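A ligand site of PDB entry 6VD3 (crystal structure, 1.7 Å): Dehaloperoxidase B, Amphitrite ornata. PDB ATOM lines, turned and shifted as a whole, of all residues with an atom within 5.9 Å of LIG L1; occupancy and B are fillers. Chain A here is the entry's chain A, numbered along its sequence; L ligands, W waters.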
ATOM      1  N   PHE A  21       2.492   3.876 -12.774  1.00  0.00           N
ATOM      2  CA  PHE A  21       1.894   4.944 -11.922  1.00  0.00           C
ATOM      3  C   PHE A  21       1.007   4.265 -10.859  1.00  0.00           C
ATOM      4  O   PHE A  21       0.992   4.726  -9.729  1.00  0.00           O
ATOM      5  CB  PHE A  21       1.142   5.966 -12.764  1.00  0.00           C
ATOM      6  CG  PHE A  21       0.577   7.152 -12.013  1.00  0.00           C
ATOM      7  CD1 PHE A  21       1.348   7.852 -11.113  1.00  0.00           C
ATOM      8  CD2 PHE A  21      -0.770   7.487 -12.122  1.00  0.00           C
ATOM      9  CE1 PHE A  21       0.816   8.948 -10.424  1.00  0.00           C
ATOM     10  CE2 PHE A  21      -1.301   8.588 -11.456  1.00  0.00           C
ATOM     11  CZ  PHE A  21      -0.505   9.311 -10.585  1.00  0.00           C
ATOM     12  N   PHE A  24       3.153   3.043  -8.188  1.00  0.00           N
ATOM     13  CA  PHE A  24       3.615   4.200  -7.385  1.00  0.00           C
ATOM     14  C   PHE A  24       2.527   4.573  -6.379  1.00  0.00           C
ATOM     15  O   PHE A  24       2.861   4.679  -5.170  1.00  0.00           O
ATOM     16  CB  PHE A  24       4.024   5.324  -8.341  1.00  0.00           C
ATOM     17  CG  PHE A  24       4.132   6.693  -7.723  1.00  0.00           C
ATOM     18  CD1 PHE A  24       5.186   7.027  -6.873  1.00  0.00           C
ATOM     19  CD2 PHE A  24       3.185   7.678  -7.998  1.00  0.00           C
ATOM     20  CE1 PHE A  24       5.343   8.323  -6.386  1.00  0.00           C
ATOM     21  CE2 PHE A  24       3.300   8.961  -7.480  1.00  0.00           C
ATOM     22  CZ  PHE A  24       4.373   9.273  -6.660  1.00  0.00           C
ATOM     23  N   GLU A  31       0.719   9.978  -1.812  1.00  0.00           N
ATOM     24  CA  GLU A  31       0.961  10.687  -3.090  1.00  0.00           C
ATOM     25  C   GLU A  31      -0.385  11.073  -3.759  1.00  0.00           C
ATOM     26  O   GLU A  31      -0.366  12.004  -4.556  1.00  0.00           O
ATOM     27  CB  GLU A  31       1.916   9.875  -3.972  1.00  0.00           C
ATOM     28  CG  GLU A  31       3.316   9.742  -3.363  1.00  0.00           C
ATOM     29  CD  GLU A  31       4.136  11.029  -3.354  1.00  0.00           C
ATOM     30  OE1 GLU A  31       4.810  11.349  -2.340  1.00  0.00           O
ATOM     31  OE2 GLU A  31       4.084  11.751  -4.366  1.00  0.00           O
ATOM     32  N   ASN A  34      -1.885  14.914  -4.232  1.00  0.00           N
ATOM     33  CA  ASN A  34      -1.719  15.720  -5.471  1.00  0.00           C
ATOM     34  C   ASN A  34      -2.702  15.267  -6.552  1.00  0.00           C
ATOM     35  O   ASN A  34      -2.770  15.947  -7.574  1.00  0.00           O
ATOM     36  CB  ASN A  34      -0.276  15.700  -5.984  1.00  0.00           C
ATOM     37  CG  ASN A  34       0.643  16.480  -5.077  1.00  0.00           C
ATOM     38  OD1 ASN A  34       0.379  17.649  -4.781  1.00  0.00           O
ATOM     39  ND2 ASN A  34       1.712  15.843  -4.624  1.00  0.00           N
ATOM     40  N   PHE A  35      -3.463  14.188  -6.332  1.00  0.00           N
ATOM     41  CA  PHE A  35      -4.441  13.656  -7.306  1.00  0.00           C
ATOM     42  C   PHE A  35      -5.769  13.389  -6.585  1.00  0.00           C
ATOM     43  O   PHE A  35      -6.225  12.251  -6.562  1.00  0.00           O
ATOM     44  CB  PHE A  35      -3.860  12.392  -7.962  1.00  0.00           C
ATOM     45  CG  PHE A  35      -2.485  12.604  -8.536  1.00  0.00           C
ATOM     46  CD1 PHE A  35      -2.321  13.173  -9.791  1.00  0.00           C
ATOM     47  CD2 PHE A  35      -1.348  12.257  -7.810  1.00  0.00           C
ATOM     48  CE1 PHE A  35      -1.060  13.354 -10.336  1.00  0.00           C
ATOM     49  CE2 PHE A  35      -0.083  12.462  -8.350  1.00  0.00           C
ATOM     50  CZ  PHE A  35       0.054  13.026  -9.599  1.00  0.00           C
ATOM     51  N   TYR A  38      -8.400  10.919  -7.716  1.00  0.00           N
ATOM     52  CA  TYR A  38      -7.988   9.492  -7.806  1.00  0.00           C
ATOM     53  C   TYR A  38      -8.237   8.784  -6.464  1.00  0.00           C
ATOM     54  O   TYR A  38      -8.085   7.542  -6.371  1.00  0.00           O
ATOM     55  CB  TYR A  38      -6.552   9.369  -8.308  1.00  0.00           C
ATOM     56  CG  TYR A  38      -6.292   9.951  -9.679  1.00  0.00           C
ATOM     57  CD1 TYR A  38      -7.328  10.233 -10.559  1.00  0.00           C
ATOM     58  CD2 TYR A  38      -4.999  10.169 -10.124  1.00  0.00           C
ATOM     59  CE1 TYR A  38      -7.090  10.768 -11.813  1.00  0.00           C
ATOM     60  CE2 TYR A  38      -4.745  10.709 -11.371  1.00  0.00           C
ATOM     61  CZ  TYR A  38      -5.789  10.976 -12.236  1.00  0.00           C
ATOM     62  OH  TYR A  38      -5.595  11.517 -13.482  1.00  0.00           O
ATOM     63  N   ASP A  54      -5.112   9.646 -19.965  1.00  0.00           N
ATOM     64  CA  ASP A  54      -4.544  10.727 -20.821  1.00  0.00           C
ATOM     65  C   ASP A  54      -3.323  11.355 -20.135  1.00  0.00           C
ATOM     66  O   ASP A  54      -2.253  11.439 -20.788  1.00  0.00           O
ATOM     67  CB  ASP A  54      -5.588  11.773 -21.171  1.00  0.00           C
ATOM     68  CG  ASP A  54      -5.074  12.807 -22.163  1.00  0.00           C
ATOM     69  OD1 ASP A  54      -4.656  12.389 -23.249  1.00  0.00           O
ATOM     70  OD2 ASP A  54      -5.060  14.012 -21.817  1.00  0.00           O
ATOM     71  N   HIS A  55      -3.460  11.777 -18.868  1.00  0.00           N
ATOM     72  CA  HIS A  55      -2.365  12.479 -18.128  1.00  0.00           C
ATOM     73  C   HIS A  55      -1.216  11.513 -17.857  1.00  0.00           C
ATOM     74  O   HIS A  55      -0.032  11.814 -18.108  1.00  0.00           O
ATOM     75  CB  HIS A  55      -2.915  13.113 -16.859  1.00  0.00           C
ATOM     76  CG  HIS A  55      -3.855  14.250 -17.102  1.00  0.00           C
ATOM     77  ND1 HIS A  55      -3.690  15.466 -16.467  1.00  0.00           N
ATOM     78  CD2 HIS A  55      -4.915  14.396 -17.920  1.00  0.00           C
ATOM     79  CE1 HIS A  55      -4.652  16.293 -16.844  1.00  0.00           C
ATOM     80  NE2 HIS A  55      -5.400  15.665 -17.742  1.00  0.00           N
ATOM     81  N   THR A  56      -1.498  10.285 -17.468  1.00  0.00           N
ATOM     82  CA  THR A  56      -0.397   9.328 -17.147  1.00  0.00           C
ATOM     83  C   THR A  56       0.413   9.073 -18.409  1.00  0.00           C
ATOM     84  O   THR A  56       1.629   9.034 -18.320  1.00  0.00           O
ATOM     85  CB  THR A  56      -0.900   7.982 -16.607  1.00  0.00           C
ATOM     86  OG1 THR A  56      -1.736   7.377 -17.606  1.00  0.00           O
ATOM     87  CG2 THR A  56      -1.635   8.181 -15.299  1.00  0.00           C
ATOM     88  N   LYS A  58       0.795  11.043 -21.081  1.00  0.00           N
ATOM     89  CA  LYS A  58       1.567  12.263 -21.414  1.00  0.00           C
ATOM     90  C   LYS A  58       2.780  12.411 -20.488  1.00  0.00           C
ATOM     91  O   LYS A  58       3.845  12.813 -20.962  1.00  0.00           O
ATOM     92  CB  LYS A  58       0.622  13.449 -21.365  1.00  0.00           C
ATOM     93  CG  LYS A  58      -0.258  13.571 -22.588  1.00  0.00           C
ATOM     94  CD  LYS A  58      -1.336  14.635 -22.457  1.00  0.00           C
ATOM     95  CE  LYS A  58      -2.413  14.565 -23.520  1.00  0.00           C
ATOM     96  NZ  LYS A  58      -3.325  15.749 -23.487  1.00  0.00           N
ATOM     97  N   VAL A  59       2.633  12.084 -19.210  1.00  0.00           N
ATOM     98  CA  VAL A  59       3.751  12.098 -18.238  1.00  0.00           C
ATOM     99  C   VAL A  59       4.810  11.104 -18.722  1.00  0.00           C
ATOM    100  O   VAL A  59       6.020  11.479 -18.805  1.00  0.00           O
ATOM    101  CB  VAL A  59       3.318  11.756 -16.804  1.00  0.00           C
ATOM    102  CG1 VAL A  59       4.543  11.632 -15.901  1.00  0.00           C
ATOM    103  CG2 VAL A  59       2.388  12.792 -16.241  1.00  0.00           C
ATOM    104  N   PHE A  60       4.407   9.894 -19.081  1.00  0.00           N
ATOM    105  CA  PHE A  60       5.395   8.855 -19.500  1.00  0.00           C
ATOM    106  C   PHE A  60       5.955   9.167 -20.892  1.00  0.00           C
ATOM    107  O   PHE A  60       7.167   8.926 -21.137  1.00  0.00           O
ATOM    108  CB  PHE A  60       4.755   7.484 -19.415  1.00  0.00           C
ATOM    109  CG  PHE A  60       4.934   6.912 -18.032  1.00  0.00           C
ATOM    110  CD1 PHE A  60       4.168   7.388 -16.989  1.00  0.00           C
ATOM    111  CD2 PHE A  60       5.924   5.995 -17.769  1.00  0.00           C
ATOM    112  CE1 PHE A  60       4.327   6.870 -15.706  1.00  0.00           C
ATOM    113  CE2 PHE A  60       6.140   5.544 -16.469  1.00  0.00           C
ATOM    114  CZ  PHE A  60       5.313   5.966 -15.444  1.00  0.00           C
ATOM    115  N   LEU A  62       6.694  12.147 -21.983  1.00  0.00           N
ATOM    116  CA  LEU A  62       7.806  13.100 -21.722  1.00  0.00           C
ATOM    117  C   LEU A  62       8.946  12.422 -20.954  1.00  0.00           C
ATOM    118  O   LEU A  62      10.142  12.709 -21.225  1.00  0.00           O
ATOM    119  CB  LEU A  62       7.290  14.321 -20.957  1.00  0.00           C
ATOM    120  CG  LEU A  62       8.359  15.396 -20.741  1.00  0.00           C
ATOM    121  CD1 LEU A  62       9.055  15.776 -22.039  1.00  0.00           C
ATOM    122  CD2 LEU A  62       7.740  16.601 -20.077  1.00  0.00           C
ATOM    123  N   MET A  63       8.645  11.520 -20.011  1.00  0.00           N
ATOM    124  CA  MET A  63       9.719  10.801 -19.273  1.00  0.00           C
ATOM    125  C   MET A  63      10.583  10.070 -20.308  1.00  0.00           C
ATOM    126  O   MET A  63      11.820  10.094 -20.173  1.00  0.00           O
ATOM    127  CB  MET A  63       9.145   9.800 -18.254  1.00  0.00           C
ATOM    128  CG  MET A  63      10.168   9.229 -17.274  1.00  0.00           C
ATOM    129  SD  MET A  63       9.676   7.594 -16.618  1.00  0.00           S
ATOM    130  CE  MET A  63       8.661   7.916 -15.172  1.00  0.00           C
ATOM    131  N   VAL A  66      12.858  12.484 -22.127  1.00  0.00           N
ATOM    132  CA  VAL A  66      13.963  12.906 -21.211  1.00  0.00           C
ATOM    133  C   VAL A  66      15.001  11.788 -21.095  1.00  0.00           C
ATOM    134  O   VAL A  66      16.219  12.048 -21.179  1.00  0.00           O
ATOM    135  CB  VAL A  66      13.389  13.383 -19.864  1.00  0.00           C
ATOM    136  CG1 VAL A  66      14.500  13.621 -18.861  1.00  0.00           C
ATOM    137  CG2 VAL A  66      12.484  14.617 -20.009  1.00  0.00           C
ATOM    138  N   LEU A  83      11.105  20.566 -16.185  1.00  0.00           N
ATOM    139  CA  LEU A  83      10.339  19.821 -15.166  1.00  0.00           C
ATOM    140  C   LEU A  83      10.233  20.675 -13.906  1.00  0.00           C
ATOM    141  O   LEU A  83       9.193  20.636 -13.247  1.00  0.00           O
ATOM    142  CB  LEU A  83      11.039  18.494 -14.878  1.00  0.00           C
ATOM    143  CG  LEU A  83      10.950  17.473 -16.014  1.00  0.00           C
ATOM    144  CD1 LEU A  83      11.863  16.290 -15.735  1.00  0.00           C
ATOM    145  CD2 LEU A  83       9.524  16.985 -16.207  1.00  0.00           C
ATOM    146  N   MET A  86       7.620  23.875 -14.815  1.00  0.00           N
ATOM    147  CA  MET A  86       6.196  23.576 -15.180  1.00  0.00           C
ATOM    148  C   MET A  86       5.257  23.976 -14.024  1.00  0.00           C
ATOM    149  O   MET A  86       5.499  23.563 -12.862  1.00  0.00           O
ATOM    150  CB  MET A  86       5.994  22.095 -15.456  1.00  0.00           C
ATOM    151  CG  MET A  86       6.437  21.654 -16.792  1.00  0.00           C
ATOM    152  SD  MET A  86       6.463  19.844 -16.770  1.00  0.00           S
ATOM    153  CE  MET A  86       4.708  19.525 -16.627  1.00  0.00           C
ATOM    154  N   GLN A  88       2.439  22.860 -13.300  1.00  0.00           N
ATOM    155  CA  GLN A  88       1.767  21.655 -12.730  1.00  0.00           C
ATOM    156  C   GLN A  88       2.673  21.024 -11.663  1.00  0.00           C
ATOM    157  O   GLN A  88       2.140  20.206 -10.876  1.00  0.00           O
ATOM    158  CB  GLN A  88       1.360  20.714 -13.857  1.00  0.00           C
ATOM    159  CG  GLN A  88       0.060  21.134 -14.522  1.00  0.00           C
ATOM    160  CD  GLN A  88      -0.027  20.685 -15.966  1.00  0.00           C
ATOM    161  OE1 GLN A  88       0.981  20.608 -16.668  1.00  0.00           O
ATOM    162  NE2 GLN A  88      -1.248  20.413 -16.419  1.00  0.00           N
ATOM    163  N   HIS A  89       3.948  21.408 -11.596  1.00  0.00           N
ATOM    164  CA  HIS A  89       4.949  20.896 -10.623  1.00  0.00           C
ATOM    165  C   HIS A  89       5.242  21.902  -9.516  1.00  0.00           C
ATOM    166  O   HIS A  89       6.182  21.613  -8.730  1.00  0.00           O
ATOM    167  CB  HIS A  89       6.252  20.517 -11.307  1.00  0.00           C
ATOM    168  CG  HIS A  89       6.083  19.321 -12.153  1.00  0.00           C
ATOM    169  ND1 HIS A  89       6.986  18.969 -13.114  1.00  0.00           N
ATOM    170  CD2 HIS A  89       5.070  18.424 -12.239  1.00  0.00           C
ATOM    171  CE1 HIS A  89       6.558  17.879 -13.719  1.00  0.00           C
ATOM    172  NE2 HIS A  89       5.410  17.524 -13.185  1.00  0.00           N
ATOM    173  N   LEU A  92       5.707  20.450  -5.902  1.00  0.00           N
ATOM    174  CA  LEU A  92       6.456  19.177  -5.729  1.00  0.00           C
ATOM    175  C   LEU A  92       7.851  19.426  -5.161  1.00  0.00           C
ATOM    176  O   LEU A  92       8.380  20.543  -5.299  1.00  0.00           O
ATOM    177  CB  LEU A  92       6.556  18.470  -7.078  1.00  0.00           C
ATOM    178  CG  LEU A  92       5.226  18.190  -7.768  1.00  0.00           C
ATOM    179  CD1 LEU A  92       5.447  17.363  -9.025  1.00  0.00           C
ATOM    180  CD2 LEU A  92       4.230  17.504  -6.827  1.00  0.00           C
ATOM    181  N   ASN A  96       9.053  13.407  -4.351  1.00  0.00           N
ATOM    182  CA  ASN A  96       7.951  12.892  -5.209  1.00  0.00           C
ATOM    183  C   ASN A  96       8.540  12.085  -6.370  1.00  0.00           C
ATOM    184  O   ASN A  96       8.010  11.041  -6.693  1.00  0.00           O
ATOM    185  CB  ASN A  96       7.012  13.990  -5.726  1.00  0.00           C
ATOM    186  CG  ASN A  96       6.354  14.808  -4.625  1.00  0.00           C
ATOM    187  OD1 ASN A  96       6.764  15.952  -4.380  1.00  0.00           O
ATOM    188  ND2 ASN A  96       5.350  14.256  -3.968  1.00  0.00           N
ATOM    189  N   PHE A  97       9.601  12.595  -7.010  1.00  0.00           N
ATOM    190  CA  PHE A  97      10.257  11.984  -8.191  1.00  0.00           C
ATOM    191  C   PHE A  97      11.070  10.740  -7.766  1.00  0.00           C
ATOM    192  O   PHE A  97      11.086   9.722  -8.498  1.00  0.00           O
ATOM    193  CB  PHE A  97      11.159  13.040  -8.852  1.00  0.00           C
ATOM    194  CG  PHE A  97      10.373  14.133  -9.503  1.00  0.00           C
ATOM    195  CD1 PHE A  97       9.906  15.214  -8.773  1.00  0.00           C
ATOM    196  CD2 PHE A  97      10.095  14.093 -10.851  1.00  0.00           C
ATOM    197  CE1 PHE A  97       9.138  16.200  -9.377  1.00  0.00           C
ATOM    198  CE2 PHE A  97       9.372  15.111 -11.459  1.00  0.00           C
ATOM    199  CZ  PHE A  97       8.855  16.132 -10.708  1.00  0.00           C
ATOM    200  N   LEU A 100       8.603   7.894  -7.351  1.00  0.00           N
ATOM    201  CA  LEU A 100       8.149   7.379  -8.655  1.00  0.00           C
ATOM    202  C   LEU A 100       9.198   6.416  -9.215  1.00  0.00           C
ATOM    203  O   LEU A 100       8.832   5.329  -9.689  1.00  0.00           O
ATOM    204  CB  LEU A 100       7.877   8.543  -9.602  1.00  0.00           C
ATOM    205  CG  LEU A 100       7.486   8.137 -11.012  1.00  0.00           C
ATOM    206  CD1 LEU A 100       6.175   7.367 -11.060  1.00  0.00           C
ATOM    207  CD2 LEU A 100       7.420   9.368 -11.881  1.00  0.00           C
ATOM    208  N   PHE A 101      10.479   6.774  -9.175  1.00  0.00           N
ATOM    209  CA  PHE A 101      11.571   5.957  -9.804  1.00  0.00           C
ATOM    210  C   PHE A 101      11.814   4.723  -8.941  1.00  0.00           C
ATOM    211  O   PHE A 101      12.142   3.688  -9.536  1.00  0.00           O
ATOM    212  CB  PHE A 101      12.781   6.823 -10.149  1.00  0.00           C
ATOM    213  CG  PHE A 101      12.521   7.535 -11.448  1.00  0.00           C
ATOM    214  CD1 PHE A 101      12.768   6.927 -12.660  1.00  0.00           C
ATOM    215  CD2 PHE A 101      11.911   8.767 -11.477  1.00  0.00           C
ATOM    216  CE1 PHE A 101      12.475   7.559 -13.854  1.00  0.00           C
ATOM    217  CE2 PHE A 101      11.622   9.422 -12.666  1.00  0.00           C
ATOM    218  CZ  PHE A 101      11.897   8.799 -13.870  1.00  0.00           C
ATOM    219  N   LEU A 127      18.182  12.134 -12.196  1.00  0.00           N
ATOM    220  CA  LEU A 127      17.072  13.071 -12.480  1.00  0.00           C
ATOM    221  C   LEU A 127      16.785  13.889 -11.228  1.00  0.00           C
ATOM    222  O   LEU A 127      16.757  15.124 -11.367  1.00  0.00           O
ATOM    223  CB  LEU A 127      15.817  12.348 -12.954  1.00  0.00           C
ATOM    224  CG  LEU A 127      14.603  13.248 -13.178  1.00  0.00           C
ATOM    225  CD1 LEU A 127      14.906  14.380 -14.166  1.00  0.00           C
ATOM    226  CD2 LEU A 127      13.410  12.413 -13.613  1.00  0.00           C
HETATM  227  C1  LIG L   1       1.402  17.040 -14.986  1.00  0.00           C
HETATM  228  C2  LIG L   1       5.593  15.503 -16.813  1.00  0.00           C
HETATM  229  C3  LIG L   1       6.849  13.679 -12.543  1.00  0.00           C
HETATM  230  C4  LIG L   1       2.845  15.548 -10.652  1.00  0.00           C
HETATM  231  C5  LIG L   1       2.359  16.659 -15.931  1.00  0.00           C
HETATM  232  C6  LIG L   1       2.256  16.714 -17.365  1.00  0.00           C
HETATM  233  C7  LIG L   1       3.436  16.289 -17.859  1.00  0.00           C
HETATM  234  C8  LIG L   1       4.272  15.932 -16.768  1.00  0.00           C
HETATM  235  C9  LIG L   1       3.787  16.183 -19.325  1.00  0.00           C
HETATM  236  C10 LIG L   1       1.058  17.209 -18.127  1.00  0.00           C
HETATM  237  C11 LIG L   1      -0.045  16.167 -18.270  1.00  0.00           C
HETATM  238  C12 LIG L   1      -1.162  16.635 -19.148  1.00  0.00           C
HETATM  239  O1  LIG L   1      -1.232  17.755 -19.609  1.00  0.00           O
HETATM  240  O2  LIG L   1      -2.073  15.729 -19.367  1.00  0.00           O
HETATM  241  C13 LIG L   1       6.270  14.741 -15.881  1.00  0.00           C
HETATM  242  C14 LIG L   1       7.431  13.942 -16.091  1.00  0.00           C
HETATM  243  C15 LIG L   1       7.800  13.408 -14.900  1.00  0.00           C
HETATM  244  C16 LIG L   1       6.872  13.919 -13.914  1.00  0.00           C
HETATM  245  C17 LIG L   1       8.095  13.692 -17.427  1.00  0.00           C
HETATM  246  C18 LIG L   1       8.962  12.500 -14.653  1.00  0.00           C
HETATM  247  C19 LIG L   1       8.653  11.382 -13.709  1.00  0.00           C
HETATM  248  C20 LIG L   1       5.850  13.964 -11.633  1.00  0.00           C
HETATM  249  C21 LIG L   1       5.792  13.561 -10.265  1.00  0.00           C
HETATM  250  C22 LIG L   1       4.664  14.057  -9.712  1.00  0.00           C
HETATM  251  C23 LIG L   1       3.994  14.811 -10.768  1.00  0.00           C
HETATM  252  C24 LIG L   1       6.803  12.696  -9.569  1.00  0.00           C
HETATM  253  C25 LIG L   1       4.162  13.887  -8.297  1.00  0.00           C
HETATM  254  C26 LIG L   1       3.666  12.474  -8.025  1.00  0.00           C
HETATM  255  C27 LIG L   1       2.092  16.146 -11.631  1.00  0.00           C
HETATM  256  C28 LIG L   1       0.874  16.825 -11.447  1.00  0.00           C
HETATM  257  C29 LIG L   1       0.415  17.260 -12.663  1.00  0.00           C
HETATM  258  C30 LIG L   1       1.426  16.837 -13.632  1.00  0.00           C
HETATM  259  C31 LIG L   1       0.175  17.042 -10.129  1.00  0.00           C
HETATM  260  C32 LIG L   1      -0.817  18.071 -12.970  1.00  0.00           C
HETATM  261  C33 LIG L   1      -2.122  17.399 -12.550  1.00  0.00           C
HETATM  262  C34 LIG L   1      -2.329  16.062 -13.185  1.00  0.00           C
HETATM  263  O3  LIG L   1      -1.741  15.951 -14.355  1.00  0.00           O
HETATM  264  O4  LIG L   1      -2.999  15.163 -12.686  1.00  0.00           O
HETATM  265  N1  LIG L   1       3.614  16.191 -15.580  1.00  0.00           N
HETATM  266  N2  LIG L   1       5.965  14.768 -14.534  1.00  0.00           N
HETATM  267  N3  LIG L   1       4.760  14.767 -11.916  1.00  0.00           N
HETATM  268  N4  LIG L   1       2.436  16.158 -12.972  1.00  0.00           N
HETATM  269 FE1  LIG L   1       4.306  15.647 -13.717  1.00  0.00          FE
HETATM  270  O1  LG2 L   2      -1.358  13.005 -14.198  1.00  0.00           O
HETATM  271  C1  LG2 L   2      -0.190  12.448 -13.760  1.00  0.00           C
HETATM  272  C2  LG2 L   2       0.033  11.087 -13.897  1.00  0.00           C
HETATM  273  C3  LG2 L   2       1.212  10.527 -13.451  1.00  0.00           C
HETATM  274  C4  LG2 L   2       2.163  11.341 -12.869  1.00  0.00           C
HETATM  275  C5  LG2 L   2       1.947  12.692 -12.711  1.00  0.00           C
HETATM  276  C6  LG2 L   2       0.768  13.252 -13.157  1.00  0.00           C
HETATM  277 BR1  LG2 L   2       3.791  10.587 -12.260  1.00  0.00          BR
HETATM  278  O   HOH W   1       0.978  19.245 -20.967  1.00  0.00           O
HETATM  279  O   HOH W   2       2.118  13.336  -5.378  1.00  0.00           O
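A ring nitrogen (ND1) of His 55 sits at hydrogen-bond distance from an oxygen (O3) of LIG L1, 2.9 Å away.
FE1 of LIG L1 is bound by NE2 of His 89 (2.2 Å).
An oxygen (O3) of LIG L1 lies within hydrogen-bond range of an oxygen (O1) of LG2 L2 (3.0 Å).
The side-chain amino group (NZ) of Lys 58 is in salt-bridge range of the side-chain carboxylate (OD2) of Asp 54 (3.0 Å).
ND1 of His 89 sits close to SD of Met 86, 3.8 Å away.
The backbone carbonyl oxygen of Leu 83 lies within hydrogen-bond range of a ring nitrogen (ND1) of His 89 (2.8 Å).
The side-chain carboxylate (OE2) of Glu 31 is in hydrogen-bond range of the side-chain amide nitrogen (ND2) of Asn 96 (2.8 Å).
Phe 24 touches LIG L1 (CZ to C26, 3.6 Å).
OE2 of Glu 31 touches C26 of LIG L1, at 3.8 Å.
Phe 35 touches LIG L1 (CE1 to O4, 3.5 Å).
CD of Lys 58 touches O2 of LIG L1, 3.4 Å away.
O of Val 59 touches C17 of LIG L1, at 3.3 Å.
Leu 62 touches LIG L1 (CB to C17, 3.7 Å).
Met 63 touches LIG L1.
Leu 83 touches LIG L1 (CD2 to C14, 3.7 Å).
Met 86 touches LIG L1.
Gln 88 touches LIG L1.
Leu 92 touches LIG L1.
O of Asn 96 touches C24 of LIG L1, at 3.5 Å.
Phe 97 touches LIG L1 (CE2 to C3, 3.1 Å).
CD2 of Leu 100 touches C19 of LIG L1, at 3.0 Å.
Phe 101 touches LIG L1.
Hydrophobic or aromatic side chains that line LIG L1: Phe 24, Phe 35, His 55, Val 59, Leu 62, Met 63, Leu 83, Met 86, His 89, Leu 92, Phe 97, Leu 100 and Phe 101.
Within 4 Å of LIG L1: Phe 24, Glu 31, Phe 35, His 55, Lys 58, Val 59, Leu 62, Met 63, Leu 83, Met 86, Gln 88, His 89, Leu 92, Asn 96, Phe 97, Leu 100 and Phe 101.
Water W2 lies within hydrogen-bond range of ND2 of Asn 34 (2.6 Å) and OE2 of Glu 31 (2.7 Å).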
